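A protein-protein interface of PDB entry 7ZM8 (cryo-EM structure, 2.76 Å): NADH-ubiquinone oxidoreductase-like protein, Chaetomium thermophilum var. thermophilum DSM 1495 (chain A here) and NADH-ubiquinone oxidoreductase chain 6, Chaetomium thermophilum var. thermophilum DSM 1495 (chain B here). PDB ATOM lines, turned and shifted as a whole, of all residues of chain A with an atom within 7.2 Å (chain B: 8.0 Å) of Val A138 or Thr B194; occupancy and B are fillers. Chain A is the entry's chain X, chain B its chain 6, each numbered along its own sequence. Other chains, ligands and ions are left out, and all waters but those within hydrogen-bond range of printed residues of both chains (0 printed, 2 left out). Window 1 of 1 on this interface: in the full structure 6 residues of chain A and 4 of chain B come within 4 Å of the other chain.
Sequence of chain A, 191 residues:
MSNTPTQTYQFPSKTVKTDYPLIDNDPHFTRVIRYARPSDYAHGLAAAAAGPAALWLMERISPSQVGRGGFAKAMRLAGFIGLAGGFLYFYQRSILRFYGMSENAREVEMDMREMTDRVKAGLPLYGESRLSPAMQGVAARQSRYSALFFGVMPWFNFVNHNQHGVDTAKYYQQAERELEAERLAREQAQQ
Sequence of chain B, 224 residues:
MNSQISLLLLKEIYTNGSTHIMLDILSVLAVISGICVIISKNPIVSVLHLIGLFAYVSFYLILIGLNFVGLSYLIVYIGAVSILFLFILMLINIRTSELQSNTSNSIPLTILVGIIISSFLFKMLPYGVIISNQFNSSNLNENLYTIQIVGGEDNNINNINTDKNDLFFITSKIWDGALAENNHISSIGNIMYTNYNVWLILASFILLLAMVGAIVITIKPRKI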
ATOM      1  N   SER A 132      -6.063  13.862  -8.333  1.00  0.00           N
ATOM      2  CA  SER A 132      -4.635  14.173  -8.057  1.00  0.00           C
ATOM      3  C   SER A 132      -4.212  13.595  -6.714  1.00  0.00           C
ATOM      4  O   SER A 132      -5.079  13.438  -5.853  1.00  0.00           O
ATOM      5  CB  SER A 132      -4.457  15.649  -8.036  1.00  0.00           C
ATOM      6  OG  SER A 132      -4.748  16.178  -6.757  1.00  0.00           O
ATOM      7  N   PRO A 133      -2.909  13.329  -6.438  1.00  0.00           N
ATOM      8  CA  PRO A 133      -2.508  12.935  -5.088  1.00  0.00           C
ATOM      9  C   PRO A 133      -3.116  13.894  -4.060  1.00  0.00           C
ATOM     10  O   PRO A 133      -3.591  13.422  -3.073  1.00  0.00           O
ATOM     11  CB  PRO A 133      -1.000  13.097  -5.160  1.00  0.00           C
ATOM     12  CG  PRO A 133      -0.666  12.639  -6.544  1.00  0.00           C
ATOM     13  CD  PRO A 133      -1.763  13.259  -7.374  1.00  0.00           C
ATOM     14  N   ALA A 134      -3.065  15.199  -4.306  1.00  0.00           N
ATOM     15  CA  ALA A 134      -3.583  16.237  -3.380  1.00  0.00           C
ATOM     16  C   ALA A 134      -5.101  16.206  -3.210  1.00  0.00           C
ATOM     17  O   ALA A 134      -5.541  16.441  -2.085  1.00  0.00           O
ATOM     18  CB  ALA A 134      -3.134  17.577  -3.866  1.00  0.00           C
ATOM     19  N   MET A 135      -5.869  16.014  -4.281  1.00  0.00           N
ATOM     20  CA  MET A 135      -7.342  15.852  -4.166  1.00  0.00           C
ATOM     21  C   MET A 135      -7.664  14.549  -3.436  1.00  0.00           C
ATOM     22  O   MET A 135      -8.658  14.521  -2.716  1.00  0.00           O
ATOM     23  CB  MET A 135      -8.026  15.909  -5.526  1.00  0.00           C
ATOM     24  CG  MET A 135      -8.143  17.308  -6.072  1.00  0.00           C
ATOM     25  SD  MET A 135      -9.080  18.383  -4.967  1.00  0.00           S
ATOM     26  CE  MET A 135      -8.977  19.941  -5.848  1.00  0.00           C
ATOM     27  N   GLN A 136      -6.878  13.504  -3.656  1.00  0.00           N
ATOM     28  CA  GLN A 136      -7.039  12.236  -2.911  1.00  0.00           C
ATOM     29  C   GLN A 136      -6.818  12.522  -1.426  1.00  0.00           C
ATOM     30  O   GLN A 136      -7.580  11.971  -0.607  1.00  0.00           O
ATOM     31  CB  GLN A 136      -6.048  11.214  -3.449  1.00  0.00           C
ATOM     32  CG  GLN A 136      -6.362  10.730  -4.851  1.00  0.00           C
ATOM     33  CD  GLN A 136      -5.276   9.816  -5.355  1.00  0.00           C
ATOM     34  OE1 GLN A 136      -4.937   8.822  -4.721  1.00  0.00           O
ATOM     35  NE2 GLN A 136      -4.729  10.141  -6.511  1.00  0.00           N
ATOM     36  N   GLY A 137      -5.839  13.361  -1.091  1.00  0.00           N
ATOM     37  CA  GLY A 137      -5.657  13.766   0.312  1.00  0.00           C
ATOM     38  C   GLY A 137      -6.836  14.540   0.864  1.00  0.00           C
ATOM     39  O   GLY A 137      -7.184  14.310   2.010  1.00  0.00           O
ATOM     40  N   VAL A 138      -7.400  15.448   0.078  1.00  0.00           N
ATOM     41  CA  VAL A 138      -8.539  16.285   0.521  1.00  0.00           C
ATOM     42  C   VAL A 138      -9.757  15.386   0.729  1.00  0.00           C
ATOM     43  O   VAL A 138     -10.459  15.563   1.731  1.00  0.00           O
ATOM     44  CB  VAL A 138      -8.786  17.459  -0.457  1.00  0.00           C
ATOM     45  CG1 VAL A 138     -10.040  18.243  -0.123  1.00  0.00           C
ATOM     46  CG2 VAL A 138      -7.591  18.385  -0.560  1.00  0.00           C
ATOM     47  N   ALA A 139     -10.026  14.501  -0.218  1.00  0.00           N
ATOM     48  CA  ALA A 139     -11.164  13.568  -0.128  1.00  0.00           C
ATOM     49  C   ALA A 139     -11.033  12.734   1.141  1.00  0.00           C
ATOM     50  O   ALA A 139     -12.005  12.624   1.877  1.00  0.00           O
ATOM     51  CB  ALA A 139     -11.188  12.710  -1.365  1.00  0.00           C
ATOM     52  N   ALA A 140      -9.863  12.160   1.367  1.00  0.00           N
ATOM     53  CA  ALA A 140      -9.617  11.316   2.550  1.00  0.00           C
ATOM     54  C   ALA A 140      -9.856  12.128   3.805  1.00  0.00           C
ATOM     55  O   ALA A 140     -10.380  11.552   4.755  1.00  0.00           O
ATOM     56  CB  ALA A 140      -8.192  10.850   2.532  1.00  0.00           C
ATOM     57  N   ARG A 141      -9.466  13.396   3.816  1.00  0.00           N
ATOM     58  CA  ARG A 141      -9.591  14.184   5.062  1.00  0.00           C
ATOM     59  C   ARG A 141     -11.051  14.588   5.278  1.00  0.00           C
ATOM     60  O   ARG A 141     -11.363  15.095   6.352  1.00  0.00           O
ATOM     61  CB  ARG A 141      -8.568  15.321   5.078  1.00  0.00           C
ATOM     62  CG  ARG A 141      -7.129  14.840   5.152  1.00  0.00           C
ATOM     63  CD  ARG A 141      -6.147  15.982   5.283  1.00  0.00           C
ATOM     64  NE  ARG A 141      -6.448  17.121   4.435  1.00  0.00           N
ATOM     65  CZ  ARG A 141      -5.857  17.375   3.277  1.00  0.00           C
ATOM     66  NH1 ARG A 141      -6.197  18.448   2.588  1.00  0.00           N
ATOM     67  NH2 ARG A 141      -4.918  16.567   2.823  1.00  0.00           N
ATOM     68  N   GLN A 142     -11.917  14.314   4.309  1.00  0.00           N
ATOM     69  CA  GLN A 142     -13.353  14.666   4.423  1.00  0.00           C
ATOM     70  C   GLN A 142     -14.162  13.435   4.835  1.00  0.00           C
ATOM     71  O   GLN A 142     -15.125  13.605   5.600  1.00  0.00           O
ATOM     72  CB  GLN A 142     -13.859  15.211   3.088  1.00  0.00           C
ATOM     73  CG  GLN A 142     -15.370  15.375   3.001  1.00  0.00           C
ATOM     74  CD  GLN A 142     -15.850  16.790   3.204  1.00  0.00           C
ATOM     75  OE1 GLN A 142     -15.214  17.596   3.871  1.00  0.00           O
ATOM     76  NE2 GLN A 142     -17.002  17.103   2.640  1.00  0.00           N
ATOM     77  N   SER A 143     -13.779  12.243   4.369  1.00  0.00           N
ATOM     78  CA  SER A 143     -14.619  11.046   4.619  1.00  0.00           C
ATOM     79  C   SER A 143     -14.100  10.177   5.768  1.00  0.00           C
ATOM     80  O   SER A 143     -14.779   9.198   6.114  1.00  0.00           O
ATOM     81  CB  SER A 143     -14.788  10.279   3.344  1.00  0.00           C
ATOM     82  OG  SER A 143     -15.948   9.461   3.393  1.00  0.00           O
ATOM     83  N   TRP A 155     -22.384  11.540   4.024  1.00  0.00           N
ATOM     84  CA  TRP A 155     -21.162  11.577   3.177  1.00  0.00           C
ATOM     85  C   TRP A 155     -20.775  10.158   2.814  1.00  0.00           C
ATOM     86  O   TRP A 155     -20.916   9.296   3.670  1.00  0.00           O
ATOM     87  CB  TRP A 155     -19.991  12.315   3.839  1.00  0.00           C
ATOM     88  CG  TRP A 155     -18.985  12.766   2.826  1.00  0.00           C
ATOM     89  CD1 TRP A 155     -17.820  12.143   2.485  1.00  0.00           C
ATOM     90  CD2 TRP A 155     -19.092  13.913   1.965  1.00  0.00           C
ATOM     91  NE1 TRP A 155     -17.190  12.828   1.484  1.00  0.00           N
ATOM     92  CE2 TRP A 155     -17.945  13.919   1.145  1.00  0.00           C
ATOM     93  CE3 TRP A 155     -20.033  14.938   1.815  1.00  0.00           C
ATOM     94  CZ2 TRP A 155     -17.722  14.911   0.192  1.00  0.00           C
ATOM     95  CZ3 TRP A 155     -19.810  15.916   0.874  1.00  0.00           C
ATOM     96  CH2 TRP A 155     -18.667  15.902   0.075  1.00  0.00           C
ATOM     97  N   GLN A 163      -5.007   6.749   1.821  1.00  0.00           N
ATOM     98  CA  GLN A 163      -4.940   7.209   3.235  1.00  0.00           C
ATOM     99  C   GLN A 163      -6.082   6.565   4.023  1.00  0.00           C
ATOM    100  O   GLN A 163      -7.142   7.179   4.092  1.00  0.00           O
ATOM    101  CB  GLN A 163      -4.948   8.732   3.223  1.00  0.00           C
ATOM    102  CG  GLN A 163      -4.358   9.262   1.927  1.00  0.00           C
ATOM    103  CD  GLN A 163      -4.208  10.757   1.887  1.00  0.00           C
ATOM    104  OE1 GLN A 163      -4.649  11.468   2.783  1.00  0.00           O
ATOM    105  NE2 GLN A 163      -3.588  11.239   0.826  1.00  0.00           N
ATOM    106  N   ILE B 188      -9.306  31.212  -4.431  1.00  0.00           N
ATOM    107  CA  ILE B 188     -10.492  30.991  -3.556  1.00  0.00           C
ATOM    108  C   ILE B 188     -11.232  29.793  -4.114  1.00  0.00           C
ATOM    109  O   ILE B 188     -11.591  28.931  -3.339  1.00  0.00           O
ATOM    110  CB  ILE B 188     -11.387  32.249  -3.504  1.00  0.00           C
ATOM    111  CG1 ILE B 188     -10.699  33.398  -2.765  1.00  0.00           C
ATOM    112  CG2 ILE B 188     -12.738  31.929  -2.886  1.00  0.00           C
ATOM    113  CD1 ILE B 188     -11.430  34.712  -2.851  1.00  0.00           C
ATOM    114  N   GLY B 189     -11.354  29.721  -5.434  1.00  0.00           N
ATOM    115  CA  GLY B 189     -12.034  28.613  -6.113  1.00  0.00           C
ATOM    116  C   GLY B 189     -11.341  27.300  -5.883  1.00  0.00           C
ATOM    117  O   GLY B 189     -12.053  26.352  -5.585  1.00  0.00           O
ATOM    118  N   ASN B 190     -10.010  27.276  -5.877  1.00  0.00           N
ATOM    119  CA  ASN B 190      -9.228  26.038  -5.677  1.00  0.00           C
ATOM    120  C   ASN B 190      -9.596  25.404  -4.339  1.00  0.00           C
ATOM    121  O   ASN B 190      -9.566  24.180  -4.264  1.00  0.00           O
ATOM    122  CB  ASN B 190      -7.723  26.285  -5.729  1.00  0.00           C
ATOM    123  CG  ASN B 190      -7.172  26.645  -7.090  1.00  0.00           C
ATOM    124  OD1 ASN B 190      -7.856  26.542  -8.101  1.00  0.00           O
ATOM    125  ND2 ASN B 190      -5.924  27.074  -7.118  1.00  0.00           N
ATOM    126  N   ILE B 191      -9.944  26.185  -3.322  1.00  0.00           N
ATOM    127  CA  ILE B 191     -10.180  25.590  -1.972  1.00  0.00           C
ATOM    128  C   ILE B 191     -11.650  25.694  -1.550  1.00  0.00           C
ATOM    129  O   ILE B 191     -12.034  24.951  -0.637  1.00  0.00           O
ATOM    130  CB  ILE B 191      -9.225  26.262  -0.954  1.00  0.00           C
ATOM    131  CG1 ILE B 191      -9.557  27.742  -0.759  1.00  0.00           C
ATOM    132  CG2 ILE B 191      -7.776  26.058  -1.351  1.00  0.00           C
ATOM    133  CD1 ILE B 191      -9.233  28.266   0.612  1.00  0.00           C
ATOM    134  N   MET B 192     -12.449  26.537  -2.210  1.00  0.00           N
ATOM    135  CA  MET B 192     -13.807  26.835  -1.775  1.00  0.00           C
ATOM    136  C   MET B 192     -14.737  25.638  -1.925  1.00  0.00           C
ATOM    137  O   MET B 192     -15.718  25.517  -1.184  1.00  0.00           O
ATOM    138  CB  MET B 192     -14.322  28.028  -2.575  1.00  0.00           C
ATOM    139  CG  MET B 192     -15.783  28.335  -2.473  1.00  0.00           C
ATOM    140  SD  MET B 192     -16.148  29.852  -3.355  1.00  0.00           S
ATOM    141  CE  MET B 192     -17.889  29.976  -3.011  1.00  0.00           C
ATOM    142  N   TYR B 193     -14.475  24.769  -2.905  1.00  0.00           N
ATOM    143  CA  TYR B 193     -15.424  23.677  -3.205  1.00  0.00           C
ATOM    144  C   TYR B 193     -14.872  22.312  -2.820  1.00  0.00           C
ATOM    145  O   TYR B 193     -15.540  21.320  -3.074  1.00  0.00           O
ATOM    146  CB  TYR B 193     -15.809  23.713  -4.682  1.00  0.00           C
ATOM    147  CG  TYR B 193     -16.233  25.054  -5.201  1.00  0.00           C
ATOM    148  CD1 TYR B 193     -17.551  25.462  -5.123  1.00  0.00           C
ATOM    149  CD2 TYR B 193     -15.311  25.905  -5.773  1.00  0.00           C
ATOM    150  CE1 TYR B 193     -17.942  26.698  -5.598  1.00  0.00           C
ATOM    151  CE2 TYR B 193     -15.680  27.148  -6.241  1.00  0.00           C
ATOM    152  CZ  TYR B 193     -17.001  27.539  -6.161  1.00  0.00           C
ATOM    153  OH  TYR B 193     -17.361  28.751  -6.650  1.00  0.00           O
ATOM    154  N   THR B 194     -13.700  22.275  -2.186  1.00  0.00           N
ATOM    155  CA  THR B 194     -13.064  20.982  -1.821  1.00  0.00           C
ATOM    156  C   THR B 194     -12.699  20.962  -0.339  1.00  0.00           C
ATOM    157  O   THR B 194     -13.455  20.364   0.428  1.00  0.00           O
ATOM    158  CB  THR B 194     -11.868  20.680  -2.734  1.00  0.00           C
ATOM    159  OG1 THR B 194     -11.070  21.860  -2.831  1.00  0.00           O
ATOM    160  CG2 THR B 194     -12.278  20.231  -4.118  1.00  0.00           C
ATOM    161  N   ASN B 195     -11.599  21.607   0.042  1.00  0.00           N
ATOM    162  CA  ASN B 195     -11.078  21.573   1.436  1.00  0.00           C
ATOM    163  C   ASN B 195     -12.048  22.182   2.449  1.00  0.00           C
ATOM    164  O   ASN B 195     -12.198  21.592   3.528  1.00  0.00           O
ATOM    165  CB  ASN B 195      -9.755  22.339   1.523  1.00  0.00           C
ATOM    166  CG  ASN B 195      -8.652  21.820   0.628  1.00  0.00           C
ATOM    167  OD1 ASN B 195      -7.635  21.337   1.118  1.00  0.00           O
ATOM    168  ND2 ASN B 195      -8.820  21.940  -0.678  1.00  0.00           N
ATOM    169  N   TYR B 196     -12.686  23.299   2.116  1.00  0.00           N
ATOM    170  CA  TYR B 196     -13.562  24.024   3.074  1.00  0.00           C
ATOM    171  C   TYR B 196     -15.004  23.964   2.563  1.00  0.00           C
ATOM    172  O   TYR B 196     -15.745  24.929   2.800  1.00  0.00           O
ATOM    173  CB  TYR B 196     -13.039  25.440   3.309  1.00  0.00           C
ATOM    174  CG  TYR B 196     -11.625  25.519   3.827  1.00  0.00           C
ATOM    175  CD1 TYR B 196     -10.553  25.656   2.962  1.00  0.00           C
ATOM    176  CD2 TYR B 196     -11.359  25.448   5.181  1.00  0.00           C
ATOM    177  CE1 TYR B 196      -9.253  25.721   3.430  1.00  0.00           C
ATOM    178  CE2 TYR B 196     -10.065  25.513   5.667  1.00  0.00           C
ATOM    179  CZ  TYR B 196      -9.007  25.650   4.788  1.00  0.00           C
ATOM    180  OH  TYR B 196      -7.730  25.716   5.262  1.00  0.00           O
ATOM    181  N   ASN B 197     -15.393  22.865   1.911  1.00  0.00           N
ATOM    182  CA  ASN B 197     -16.741  22.736   1.288  1.00  0.00           C
ATOM    183  C   ASN B 197     -17.879  22.766   2.317  1.00  0.00           C
ATOM    184  O   ASN B 197     -19.014  23.023   1.908  1.00  0.00           O
ATOM    185  CB  ASN B 197     -16.805  21.583   0.276  1.00  0.00           C
ATOM    186  CG  ASN B 197     -16.624  20.202   0.867  1.00  0.00           C
ATOM    187  OD1 ASN B 197     -16.455  20.045   2.072  1.00  0.00           O
ATOM    188  ND2 ASN B 197     -16.660  19.190   0.017  1.00  0.00           N
ATOM    189  N   VAL B 198     -17.600  22.452   3.580  1.00  0.00           N
ATOM    190  CA  VAL B 198     -18.634  22.464   4.662  1.00  0.00           C
ATOM    191  C   VAL B 198     -19.180  23.887   4.837  1.00  0.00           C
ATOM    192  O   VAL B 198     -20.385  24.021   5.093  1.00  0.00           O
ATOM    193  CB  VAL B 198     -18.109  21.828   5.968  1.00  0.00           C
ATOM    194  CG1 VAL B 198     -18.578  22.543   7.227  1.00  0.00           C
ATOM    195  CG2 VAL B 198     -18.440  20.349   6.033  1.00  0.00           C
ATOM    196  N   TRP B 199     -18.331  24.903   4.695  1.00  0.00           N
ATOM    197  CA  TRP B 199     -18.794  26.317   4.778  1.00  0.00           C
ATOM    198  C   TRP B 199     -19.794  26.616   3.658  1.00  0.00           C
ATOM    199  O   TRP B 199     -20.761  27.331   3.931  1.00  0.00           O
ATOM    200  CB  TRP B 199     -17.615  27.291   4.740  1.00  0.00           C
ATOM    201  CG  TRP B 199     -16.640  27.153   5.866  1.00  0.00           C
ATOM    202  CD1 TRP B 199     -16.836  26.532   7.063  1.00  0.00           C
ATOM    203  CD2 TRP B 199     -15.301  27.674   5.898  1.00  0.00           C
ATOM    204  NE1 TRP B 199     -15.709  26.622   7.833  1.00  0.00           N
ATOM    205  CE2 TRP B 199     -14.750  27.315   7.145  1.00  0.00           C
ATOM    206  CE3 TRP B 199     -14.519  28.405   4.999  1.00  0.00           C
ATOM    207  CZ2 TRP B 199     -13.451  27.659   7.510  1.00  0.00           C
ATOM    208  CZ3 TRP B 199     -13.238  28.749   5.361  1.00  0.00           C
ATOM    209  CH2 TRP B 199     -12.715  28.383   6.601  1.00  0.00           C
ATOM    210  N   LEU B 200     -19.557  26.103   2.451  1.00  0.00           N
ATOM    211  CA  LEU B 200     -20.484  26.300   1.309  1.00  0.00           C
ATOM    212  C   LEU B 200     -21.818  25.632   1.630  1.00  0.00           C
ATOM    213  O   LEU B 200     -22.855  26.231   1.346  1.00  0.00           O
ATOM    214  CB  LEU B 200     -19.845  25.657   0.076  1.00  0.00           C
ATOM    215  CG  LEU B 200     -20.513  25.948  -1.265  1.00  0.00           C
ATOM    216  CD1 LEU B 200     -20.386  27.418  -1.629  1.00  0.00           C
ATOM    217  CD2 LEU B 200     -19.906  25.079  -2.351  1.00  0.00           C
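OG of Ser A132 sits at hydrogen-bond distance from N of Met A135, 2.7 Å away. O of Gly A137 sits close to NH2 of Arg A141. The backbone carbonyl oxygen (O) of Asn B190 is in hydrogen-bond range of the side-chain hydroxyl (OG1) of Thr B194 (3.1 Å). OG1 of Thr B194 is in hydrogen-bond range of ND2 of Asn B195, 3.1 Å away. The backbone carbonyl oxygen (O) of Thr B194 sits close to the side-chain amide oxygen (OD1) of Asn B197 (3.4 Å).
NE2 of Gln A142 is in hydrogen-bond range of OD1 of Asn B197, 3.0 Å away.
Printed residues of chain B that touch a printed residue of chain A: Thr B194, Asn B195 and Asn B197. Along chain B the printed residues that touch a printed residue of chain A span positions 194 to 197. Among the printed residues, no Asp or Glu carboxylate lies within 4 Å of a Lys or Arg side-chain nitrogen of the other chain.
Among the printed residues, merely in contact across the chains: Val A138 with Asn B195 (3.4 Å), Arg A141 with Asn B195 (3.5 Å), Met A135 with Thr B194 (3.7 Å), Val A138 with Thr B194 (3.8 Å) and Trp A155 with Asn B197 (3.9 Å).
Of chain B, only Thr B194 (3.8 Å) and Asn B195 (3.4 Å) come within 4 Å of Val A138. Of the printed residues of chain A, Thr B194 touches Met A135 and Val A138. No residue of chain B comes within 4 Å of Gly A137. No residue of chain B comes within 4 Å of Ala A139. Of the printed residues of chain B, Trp A155 touches Asn B197 (3.9 Å). Of the printed residues of chain B, Met A135 touches Thr B194 (3.7 Å). Of the printed residues of chain B, Arg A141 touches Asn B195 (3.5 Å). Of the printed residues of chain A, Asn B195 touches Val A138 (3.4 Å) and Arg A141 (3.5 Å).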
